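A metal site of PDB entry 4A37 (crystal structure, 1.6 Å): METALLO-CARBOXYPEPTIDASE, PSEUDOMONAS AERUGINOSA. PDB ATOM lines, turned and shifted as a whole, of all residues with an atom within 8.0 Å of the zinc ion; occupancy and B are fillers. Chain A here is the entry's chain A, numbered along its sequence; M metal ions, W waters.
NE2 of His 180 lies close to NE of Arg 231. A ring nitrogen (NE2) of His 180 lies within hydrogen-bond range of the side-chain carboxylate (OD1) of Asp 238. NE2 of His 273 is in hydrogen-bond range of OD2 of Asp 271 (2.6 Å). The backbone NH (N) of His 273 lies within hydrogen-bond range of the backbone carbonyl oxygen (O) of Ile 347 (2.8 Å). The backbone NH (N) of Gly 274 sits close to the side-chain carboxylate (OE1) of Glu 183, 3.0 Å away.
Of the 25 residues printed, 3 come within 4 Å of the zinc ion. The nearest printed residue that does not touch the zinc ion is Gly 274 (4.1 Å).
ND1 of His 180 is bound to the zinc ion (2.1 Å). The zinc ion is bound by a ring nitrogen (ND1) of His 273 (2.1 Å). The zinc ion is bound by water W1, at 2.1 Å. The side-chain carboxylate (OE1) of Glu 183 is bound to the zinc ion (2.2 Å). OE2 of Glu 183 is bound to the zinc ion (2.5 Å).
Water W1 bridges the side-chain carboxylate of Glu 348 (3.3 Å) and the backbone carbonyl oxygen of Gly 274 (3.5 Å).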
ATOM      1  N   TYR A  77      38.589 -17.048  16.135  1.00  0.00           N
ATOM      2  CA  TYR A  77      38.068 -17.087  17.490  1.00  0.00           C
ATOM      3  C   TYR A  77      38.621 -18.344  18.164  1.00  0.00           C
ATOM      4  O   TYR A  77      37.870 -19.258  18.502  1.00  0.00           O
ATOM      5  CB  TYR A  77      36.536 -17.115  17.431  1.00  0.00           C
ATOM      6  CG  TYR A  77      35.952 -16.006  16.569  1.00  0.00           C
ATOM      7  CD1 TYR A  77      36.011 -14.674  16.972  1.00  0.00           C
ATOM      8  CD2 TYR A  77      35.425 -16.284  15.308  1.00  0.00           C
ATOM      9  CE1 TYR A  77      35.560 -13.645  16.149  1.00  0.00           C
ATOM     10  CE2 TYR A  77      34.973 -15.260  14.466  1.00  0.00           C
ATOM     11  CZ  TYR A  77      35.041 -13.941  14.902  1.00  0.00           C
ATOM     12  OH  TYR A  77      34.640 -12.921  14.067  1.00  0.00           O
ATOM     13  N   GLN A 178      22.869 -15.925   7.248  1.00  0.00           N
ATOM     14  CA  GLN A 178      24.214 -16.298   6.874  1.00  0.00           C
ATOM     15  C   GLN A 178      25.065 -15.251   6.164  1.00  0.00           C
ATOM     16  O   GLN A 178      25.670 -15.529   5.116  1.00  0.00           O
ATOM     17  CB  GLN A 178      24.169 -17.593   6.048  1.00  0.00           C
ATOM     18  CG  GLN A 178      25.309 -18.560   6.383  1.00  0.00           C
ATOM     19  CD  GLN A 178      25.044 -19.984   5.928  1.00  0.00           C
ATOM     20  OE1 GLN A 178      23.941 -20.502   6.065  1.00  0.00           O
ATOM     21  NE2 GLN A 178      26.081 -20.639   5.400  1.00  0.00           N
ATOM     22  N   GLN A 179      25.125 -14.039   6.709  1.00  0.00           N
ATOM     23  CA  GLN A 179      25.988 -13.019   6.108  1.00  0.00           C
ATOM     24  C   GLN A 179      27.414 -13.523   6.275  1.00  0.00           C
ATOM     25  O   GLN A 179      28.289 -13.234   5.459  1.00  0.00           O
ATOM     26  CB  GLN A 179      25.850 -11.682   6.805  1.00  0.00           C
ATOM     27  CG  GLN A 179      24.572 -10.946   6.558  1.00  0.00           C
ATOM     28  CD  GLN A 179      24.658  -9.532   7.094  1.00  0.00           C
ATOM     29  OE1 GLN A 179      25.339  -8.680   6.518  1.00  0.00           O
ATOM     30  NE2 GLN A 179      23.982  -9.281   8.205  1.00  0.00           N
ATOM     31  N   HIS A 180      27.650 -14.226   7.377  1.00  0.00           N
ATOM     32  CA  HIS A 180      28.968 -14.818   7.637  1.00  0.00           C
ATOM     33  C   HIS A 180      28.800 -16.243   7.101  1.00  0.00           C
ATOM     34  O   HIS A 180      28.042 -17.053   7.642  1.00  0.00           O
ATOM     35  CB  HIS A 180      29.251 -14.800   9.148  1.00  0.00           C
ATOM     36  CG  HIS A 180      29.475 -13.414   9.679  1.00  0.00           C
ATOM     37  ND1 HIS A 180      28.899 -12.964  10.847  1.00  0.00           N
ATOM     38  CD2 HIS A 180      30.175 -12.369   9.178  1.00  0.00           C
ATOM     39  CE1 HIS A 180      29.231 -11.696  11.046  1.00  0.00           C
ATOM     40  NE2 HIS A 180      29.999 -11.308  10.039  1.00  0.00           N
ATOM     41  N   PRO A 181      29.509 -16.557   6.002  1.00  0.00           N
ATOM     42  CA  PRO A 181      29.430 -17.867   5.348  1.00  0.00           C
ATOM     43  C   PRO A 181      29.647 -19.130   6.165  1.00  0.00           C
ATOM     44  O   PRO A 181      29.076 -20.172   5.838  1.00  0.00           O
ATOM     45  CB  PRO A 181      30.420 -17.720   4.195  1.00  0.00           C
ATOM     46  CG  PRO A 181      31.477 -16.839   4.768  1.00  0.00           C
ATOM     47  CD  PRO A 181      30.627 -15.764   5.445  1.00  0.00           C
ATOM     48  N   GLY A 182      30.458 -19.064   7.216  1.00  0.00           N
ATOM     49  CA  GLY A 182      30.693 -20.260   8.015  1.00  0.00           C
ATOM     50  C   GLY A 182      29.581 -20.637   8.987  1.00  0.00           C
ATOM     51  O   GLY A 182      29.578 -21.716   9.561  1.00  0.00           O
ATOM     52  N   GLU A 183      28.631 -19.731   9.156  1.00  0.00           N
ATOM     53  CA  GLU A 183      27.538 -19.961  10.100  1.00  0.00           C
ATOM     54  C   GLU A 183      26.351 -20.641   9.437  1.00  0.00           C
ATOM     55  O   GLU A 183      25.260 -20.084   9.353  1.00  0.00           O
ATOM     56  CB  GLU A 183      27.164 -18.624  10.725  1.00  0.00           C
ATOM     57  CG  GLU A 183      28.324 -18.048  11.539  1.00  0.00           C
ATOM     58  CD  GLU A 183      28.203 -16.558  11.784  1.00  0.00           C
ATOM     59  OE1 GLU A 183      27.089 -16.008  11.662  1.00  0.00           O
ATOM     60  OE2 GLU A 183      29.240 -15.957  12.107  1.00  0.00           O
ATOM     61  N   MET A 185      24.311 -22.819  10.401  1.00  0.00           N
ATOM     62  CA  MET A 185      23.087 -22.981  11.185  1.00  0.00           C
ATOM     63  C   MET A 185      22.051 -21.943  10.730  1.00  0.00           C
ATOM     64  O   MET A 185      20.840 -22.149  10.894  1.00  0.00           O
ATOM     65  CB  MET A 185      23.393 -22.785  12.671  1.00  0.00           C
ATOM     66  CG  MET A 185      24.140 -21.477  12.980  1.00  0.00           C
ATOM     67  SD  MET A 185      25.935 -21.591  12.814  1.00  0.00           S
ATOM     68  CE  MET A 185      26.311 -22.547  14.338  1.00  0.00           C
ATOM     69  N   ALA A 186      22.536 -20.830  10.190  1.00  0.00           N
ATOM     70  CA  ALA A 186      21.657 -19.754   9.753  1.00  0.00           C
ATOM     71  C   ALA A 186      20.704 -20.173   8.635  1.00  0.00           C
ATOM     72  O   ALA A 186      19.510 -19.922   8.727  1.00  0.00           O
ATOM     73  CB  ALA A 186      22.485 -18.545   9.346  1.00  0.00           C
ATOM     74  N   LEU A 230      34.739 -18.429   6.315  1.00  0.00           N
ATOM     75  CA  LEU A 230      34.115 -18.322   7.623  1.00  0.00           C
ATOM     76  C   LEU A 230      33.393 -16.989   7.782  1.00  0.00           C
ATOM     77  O   LEU A 230      32.195 -16.928   8.106  1.00  0.00           O
ATOM     78  CB  LEU A 230      35.164 -18.393   8.739  1.00  0.00           C
ATOM     79  CG  LEU A 230      34.636 -17.795  10.063  1.00  0.00           C
ATOM     80  CD1 LEU A 230      33.666 -18.789  10.678  1.00  0.00           C
ATOM     81  CD2 LEU A 230      35.776 -17.507  11.042  1.00  0.00           C
ATOM     82  N   ARG A 231      34.127 -15.923   7.501  1.00  0.00           N
ATOM     83  CA  ARG A 231      33.664 -14.571   7.736  1.00  0.00           C
ATOM     84  C   ARG A 231      33.362 -13.597   6.604  1.00  0.00           C
ATOM     85  O   ARG A 231      32.473 -12.748   6.741  1.00  0.00           O
ATOM     86  CB  ARG A 231      34.690 -13.908   8.665  1.00  0.00           C
ATOM     87  CG  ARG A 231      34.249 -12.624   9.297  1.00  0.00           C
ATOM     88  CD  ARG A 231      33.412 -12.931  10.507  1.00  0.00           C
ATOM     89  NE  ARG A 231      33.037 -11.716  11.223  1.00  0.00           N
ATOM     90  CZ  ARG A 231      32.266 -11.703  12.298  1.00  0.00           C
ATOM     91  NH1 ARG A 231      31.794 -12.849  12.794  1.00  0.00           N
ATOM     92  NH2 ARG A 231      31.954 -10.563  12.872  1.00  0.00           N
ATOM     93  N   ASP A 238      33.623  -8.230   5.364  1.00  0.00           N
ATOM     94  CA  ASP A 238      32.740  -8.808   6.386  1.00  0.00           C
ATOM     95  C   ASP A 238      31.413  -8.113   6.080  1.00  0.00           C
ATOM     96  O   ASP A 238      31.244  -6.920   6.361  1.00  0.00           O
ATOM     97  CB  ASP A 238      33.197  -8.432   7.794  1.00  0.00           C
ATOM     98  CG  ASP A 238      32.296  -9.016   8.870  1.00  0.00           C
ATOM     99  OD1 ASP A 238      31.093  -9.227   8.611  1.00  0.00           O
ATOM    100  OD2 ASP A 238      32.789  -9.245  10.000  1.00  0.00           O
ATOM    101  N   ASN A 240      28.615  -8.071   7.527  1.00  0.00           N
ATOM    102  CA  ASN A 240      27.896  -7.462   8.637  1.00  0.00           C
ATOM    103  C   ASN A 240      28.596  -6.228   9.206  1.00  0.00           C
ATOM    104  O   ASN A 240      28.296  -5.813  10.328  1.00  0.00           O
ATOM    105  CB  ASN A 240      27.626  -8.468   9.742  1.00  0.00           C
ATOM    106  CG  ASN A 240      26.467  -8.041  10.625  1.00  0.00           C
ATOM    107  OD1 ASN A 240      25.497  -7.477  10.135  1.00  0.00           O
ATOM    108  ND2 ASN A 240      26.572  -8.293  11.927  1.00  0.00           N
ATOM    109  N   ARG A 241      29.522  -5.660   8.451  1.00  0.00           N
ATOM    110  CA  ARG A 241      30.231  -4.449   8.849  1.00  0.00           C
ATOM    111  C   ARG A 241      30.154  -3.498   7.652  1.00  0.00           C
ATOM    112  O   ARG A 241      30.771  -2.433   7.639  1.00  0.00           O
ATOM    113  CB  ARG A 241      31.702  -4.753   9.170  1.00  0.00           C
ATOM    114  CG  ARG A 241      31.937  -5.650  10.371  1.00  0.00           C
ATOM    115  CD  ARG A 241      31.498  -4.992  11.684  1.00  0.00           C
ATOM    116  NE  ARG A 241      31.820  -5.827  12.842  1.00  0.00           N
ATOM    117  CZ  ARG A 241      31.120  -6.900  13.236  1.00  0.00           C
ATOM    118  NH1 ARG A 241      30.035  -7.272  12.561  1.00  0.00           N
ATOM    119  NH2 ARG A 241      31.516  -7.595  14.281  1.00  0.00           N
ATOM    120  N   ASP A 271      18.347 -10.806  11.783  1.00  0.00           N
ATOM    121  CA  ASP A 271      19.588 -11.150  11.101  1.00  0.00           C
ATOM    122  C   ASP A 271      20.078 -12.430  11.775  1.00  0.00           C
ATOM    123  O   ASP A 271      20.503 -12.425  12.936  1.00  0.00           O
ATOM    124  CB  ASP A 271      20.572  -9.982  11.259  1.00  0.00           C
ATOM    125  CG  ASP A 271      21.880 -10.177  10.503  1.00  0.00           C
ATOM    126  OD1 ASP A 271      21.936 -10.968   9.545  1.00  0.00           O
ATOM    127  OD2 ASP A 271      22.851  -9.484  10.871  1.00  0.00           O
ATOM    128  N   ILE A 272      20.013 -13.535  11.038  1.00  0.00           N
ATOM    129  CA  ILE A 272      20.360 -14.845  11.566  1.00  0.00           C
ATOM    130  C   ILE A 272      21.832 -15.204  11.467  1.00  0.00           C
ATOM    131  O   ILE A 272      22.402 -15.271  10.371  1.00  0.00           O
ATOM    132  CB  ILE A 272      19.509 -15.946  10.875  1.00  0.00           C
ATOM    133  CG1 ILE A 272      18.049 -15.487  10.763  1.00  0.00           C
ATOM    134  CG2 ILE A 272      19.599 -17.241  11.669  1.00  0.00           C
ATOM    135  CD1 ILE A 272      17.381 -15.102  12.078  1.00  0.00           C
ATOM    136  N   HIS A 273      22.439 -15.492  12.622  1.00  0.00           N
ATOM    137  CA  HIS A 273      23.856 -15.821  12.737  1.00  0.00           C
ATOM    138  C   HIS A 273      24.139 -17.060  13.595  1.00  0.00           C
ATOM    139  O   HIS A 273      23.230 -17.703  14.108  1.00  0.00           O
ATOM    140  CB  HIS A 273      24.602 -14.666  13.425  1.00  0.00           C
ATOM    141  CG  HIS A 273      24.689 -13.408  12.614  1.00  0.00           C
ATOM    142  ND1 HIS A 273      25.863 -13.006  12.013  1.00  0.00           N
ATOM    143  CD2 HIS A 273      23.774 -12.439  12.352  1.00  0.00           C
ATOM    144  CE1 HIS A 273      25.676 -11.835  11.423  1.00  0.00           C
ATOM    145  NE2 HIS A 273      24.421 -11.478  11.618  1.00  0.00           N
ATOM    146  N   GLY A 274      25.434 -17.326  13.736  1.00  0.00           N
ATOM    147  CA  GLY A 274      25.928 -18.411  14.568  1.00  0.00           C
ATOM    148  C   GLY A 274      27.124 -17.856  15.354  1.00  0.00           C
ATOM    149  O   GLY A 274      27.893 -17.043  14.832  1.00  0.00           O
ATOM    150  N   ASP A 275      27.268 -18.251  16.605  1.00  0.00           N
ATOM    151  CA  ASP A 275      28.413 -17.776  17.383  1.00  0.00           C
ATOM    152  C   ASP A 275      29.270 -18.939  17.833  1.00  0.00           C
ATOM    153  O   ASP A 275      28.776 -19.906  18.410  1.00  0.00           O
ATOM    154  CB  ASP A 275      27.967 -16.981  18.621  1.00  0.00           C
ATOM    155  CG  ASP A 275      29.142 -16.336  19.345  1.00  0.00           C
ATOM    156  OD1 ASP A 275      29.719 -15.370  18.802  1.00  0.00           O
ATOM    157  OD2 ASP A 275      29.501 -16.797  20.440  1.00  0.00           O
ATOM    158  N   GLU A 276      30.565 -18.820  17.569  1.00  0.00           N
ATOM    159  CA  GLU A 276      31.535 -19.859  17.906  1.00  0.00           C
ATOM    160  C   GLU A 276      31.708 -20.132  19.405  1.00  0.00           C
ATOM    161  O   GLU A 276      31.728 -21.281  19.839  1.00  0.00           O
ATOM    162  CB  GLU A 276      32.897 -19.490  17.308  1.00  0.00           C
ATOM    163  CG  GLU A 276      32.904 -19.371  15.781  1.00  0.00           C
ATOM    164  CD  GLU A 276      32.579 -17.978  15.261  1.00  0.00           C
ATOM    165  OE1 GLU A 276      32.045 -17.129  16.018  1.00  0.00           O
ATOM    166  OE2 GLU A 276      32.830 -17.744  14.057  1.00  0.00           O
ATOM    167  N   TYR A 319      26.195 -11.267  24.183  1.00  0.00           N
ATOM    168  CA  TYR A 319      27.265 -10.293  23.988  1.00  0.00           C
ATOM    169  C   TYR A 319      27.088  -9.136  24.980  1.00  0.00           C
ATOM    170  O   TYR A 319      25.966  -8.845  25.387  1.00  0.00           O
ATOM    171  CB  TYR A 319      27.239  -9.707  22.566  1.00  0.00           C
ATOM    172  CG  TYR A 319      27.412 -10.690  21.438  1.00  0.00           C
ATOM    173  CD1 TYR A 319      28.327 -11.742  21.535  1.00  0.00           C
ATOM    174  CD2 TYR A 319      26.726 -10.518  20.236  1.00  0.00           C
ATOM    175  CE1 TYR A 319      28.559 -12.606  20.456  1.00  0.00           C
ATOM    176  CE2 TYR A 319      26.950 -11.364  19.143  1.00  0.00           C
ATOM    177  CZ  TYR A 319      27.868 -12.399  19.266  1.00  0.00           C
ATOM    178  OH  TYR A 319      28.104 -13.232  18.189  1.00  0.00           O
ATOM    179  N   THR A 346      19.698  -9.645  16.126  1.00  0.00           N
ATOM    180  CA  THR A 346      20.622 -10.578  15.511  1.00  0.00           C
ATOM    181  C   THR A 346      20.248 -11.808  16.339  1.00  0.00           C
ATOM    182  O   THR A 346      20.123 -11.709  17.565  1.00  0.00           O
ATOM    183  CB  THR A 346      22.088 -10.240  15.821  1.00  0.00           C
ATOM    184  OG1 THR A 346      22.457  -9.034  15.143  1.00  0.00           O
ATOM    185  CG2 THR A 346      23.004 -11.370  15.368  1.00  0.00           C
ATOM    186  N   ILE A 347      20.001 -12.942  15.687  1.00  0.00           N
ATOM    187  CA  ILE A 347      19.683 -14.164  16.405  1.00  0.00           C
ATOM    188  C   ILE A 347      20.947 -15.005  16.276  1.00  0.00           C
ATOM    189  O   ILE A 347      21.422 -15.250  15.170  1.00  0.00           O
ATOM    190  CB  ILE A 347      18.497 -14.920  15.771  1.00  0.00           C
ATOM    191  CG1 ILE A 347      17.231 -14.065  15.835  1.00  0.00           C
ATOM    192  CG2 ILE A 347      18.286 -16.250  16.486  1.00  0.00           C
ATOM    193  CD1 ILE A 347      16.826 -13.640  17.232  1.00  0.00           C
ATOM    194  N   GLU A 348      21.506 -15.419  17.404  1.00  0.00           N
ATOM    195  CA  GLU A 348      22.745 -16.194  17.395  1.00  0.00           C
ATOM    196  C   GLU A 348      22.582 -17.612  17.911  1.00  0.00           C
ATOM    197  O   GLU A 348      22.150 -17.810  19.049  1.00  0.00           O
ATOM    198  CB  GLU A 348      23.804 -15.484  18.237  1.00  0.00           C
ATOM    199  CG  GLU A 348      24.144 -14.058  17.798  1.00  0.00           C
ATOM    200  CD  GLU A 348      25.282 -14.001  16.809  1.00  0.00           C
ATOM    201  OE1 GLU A 348      25.871 -15.059  16.481  1.00  0.00           O
ATOM    202  OE2 GLU A 348      25.601 -12.878  16.353  1.00  0.00           O
ATOM    203  N   PHE A 351      27.724 -22.948  17.880  1.00  0.00           N
ATOM    204  CA  PHE A 351      28.416 -23.968  17.099  1.00  0.00           C
ATOM    205  C   PHE A 351      28.605 -25.170  18.017  1.00  0.00           C
ATOM    206  O   PHE A 351      28.816 -26.286  17.570  1.00  0.00           O
ATOM    207  CB  PHE A 351      29.791 -23.476  16.625  1.00  0.00           C
ATOM    208  CG  PHE A 351      29.763 -22.722  15.327  1.00  0.00           C
ATOM    209  CD1 PHE A 351      29.593 -21.347  15.305  1.00  0.00           C
ATOM    210  CD2 PHE A 351      29.912 -23.402  14.117  1.00  0.00           C
ATOM    211  CE1 PHE A 351      29.574 -20.643  14.102  1.00  0.00           C
ATOM    212  CE2 PHE A 351      29.901 -22.712  12.906  1.00  0.00           C
ATOM    213  CZ  PHE A 351      29.733 -21.331  12.903  1.00  0.00           C
HETATM  214 ZN    ZN M   1      27.700 -13.979  12.167  1.00  0.00          ZN
HETATM  215  O   HOH W   1      28.057 -13.636  14.254  1.00  0.00           O
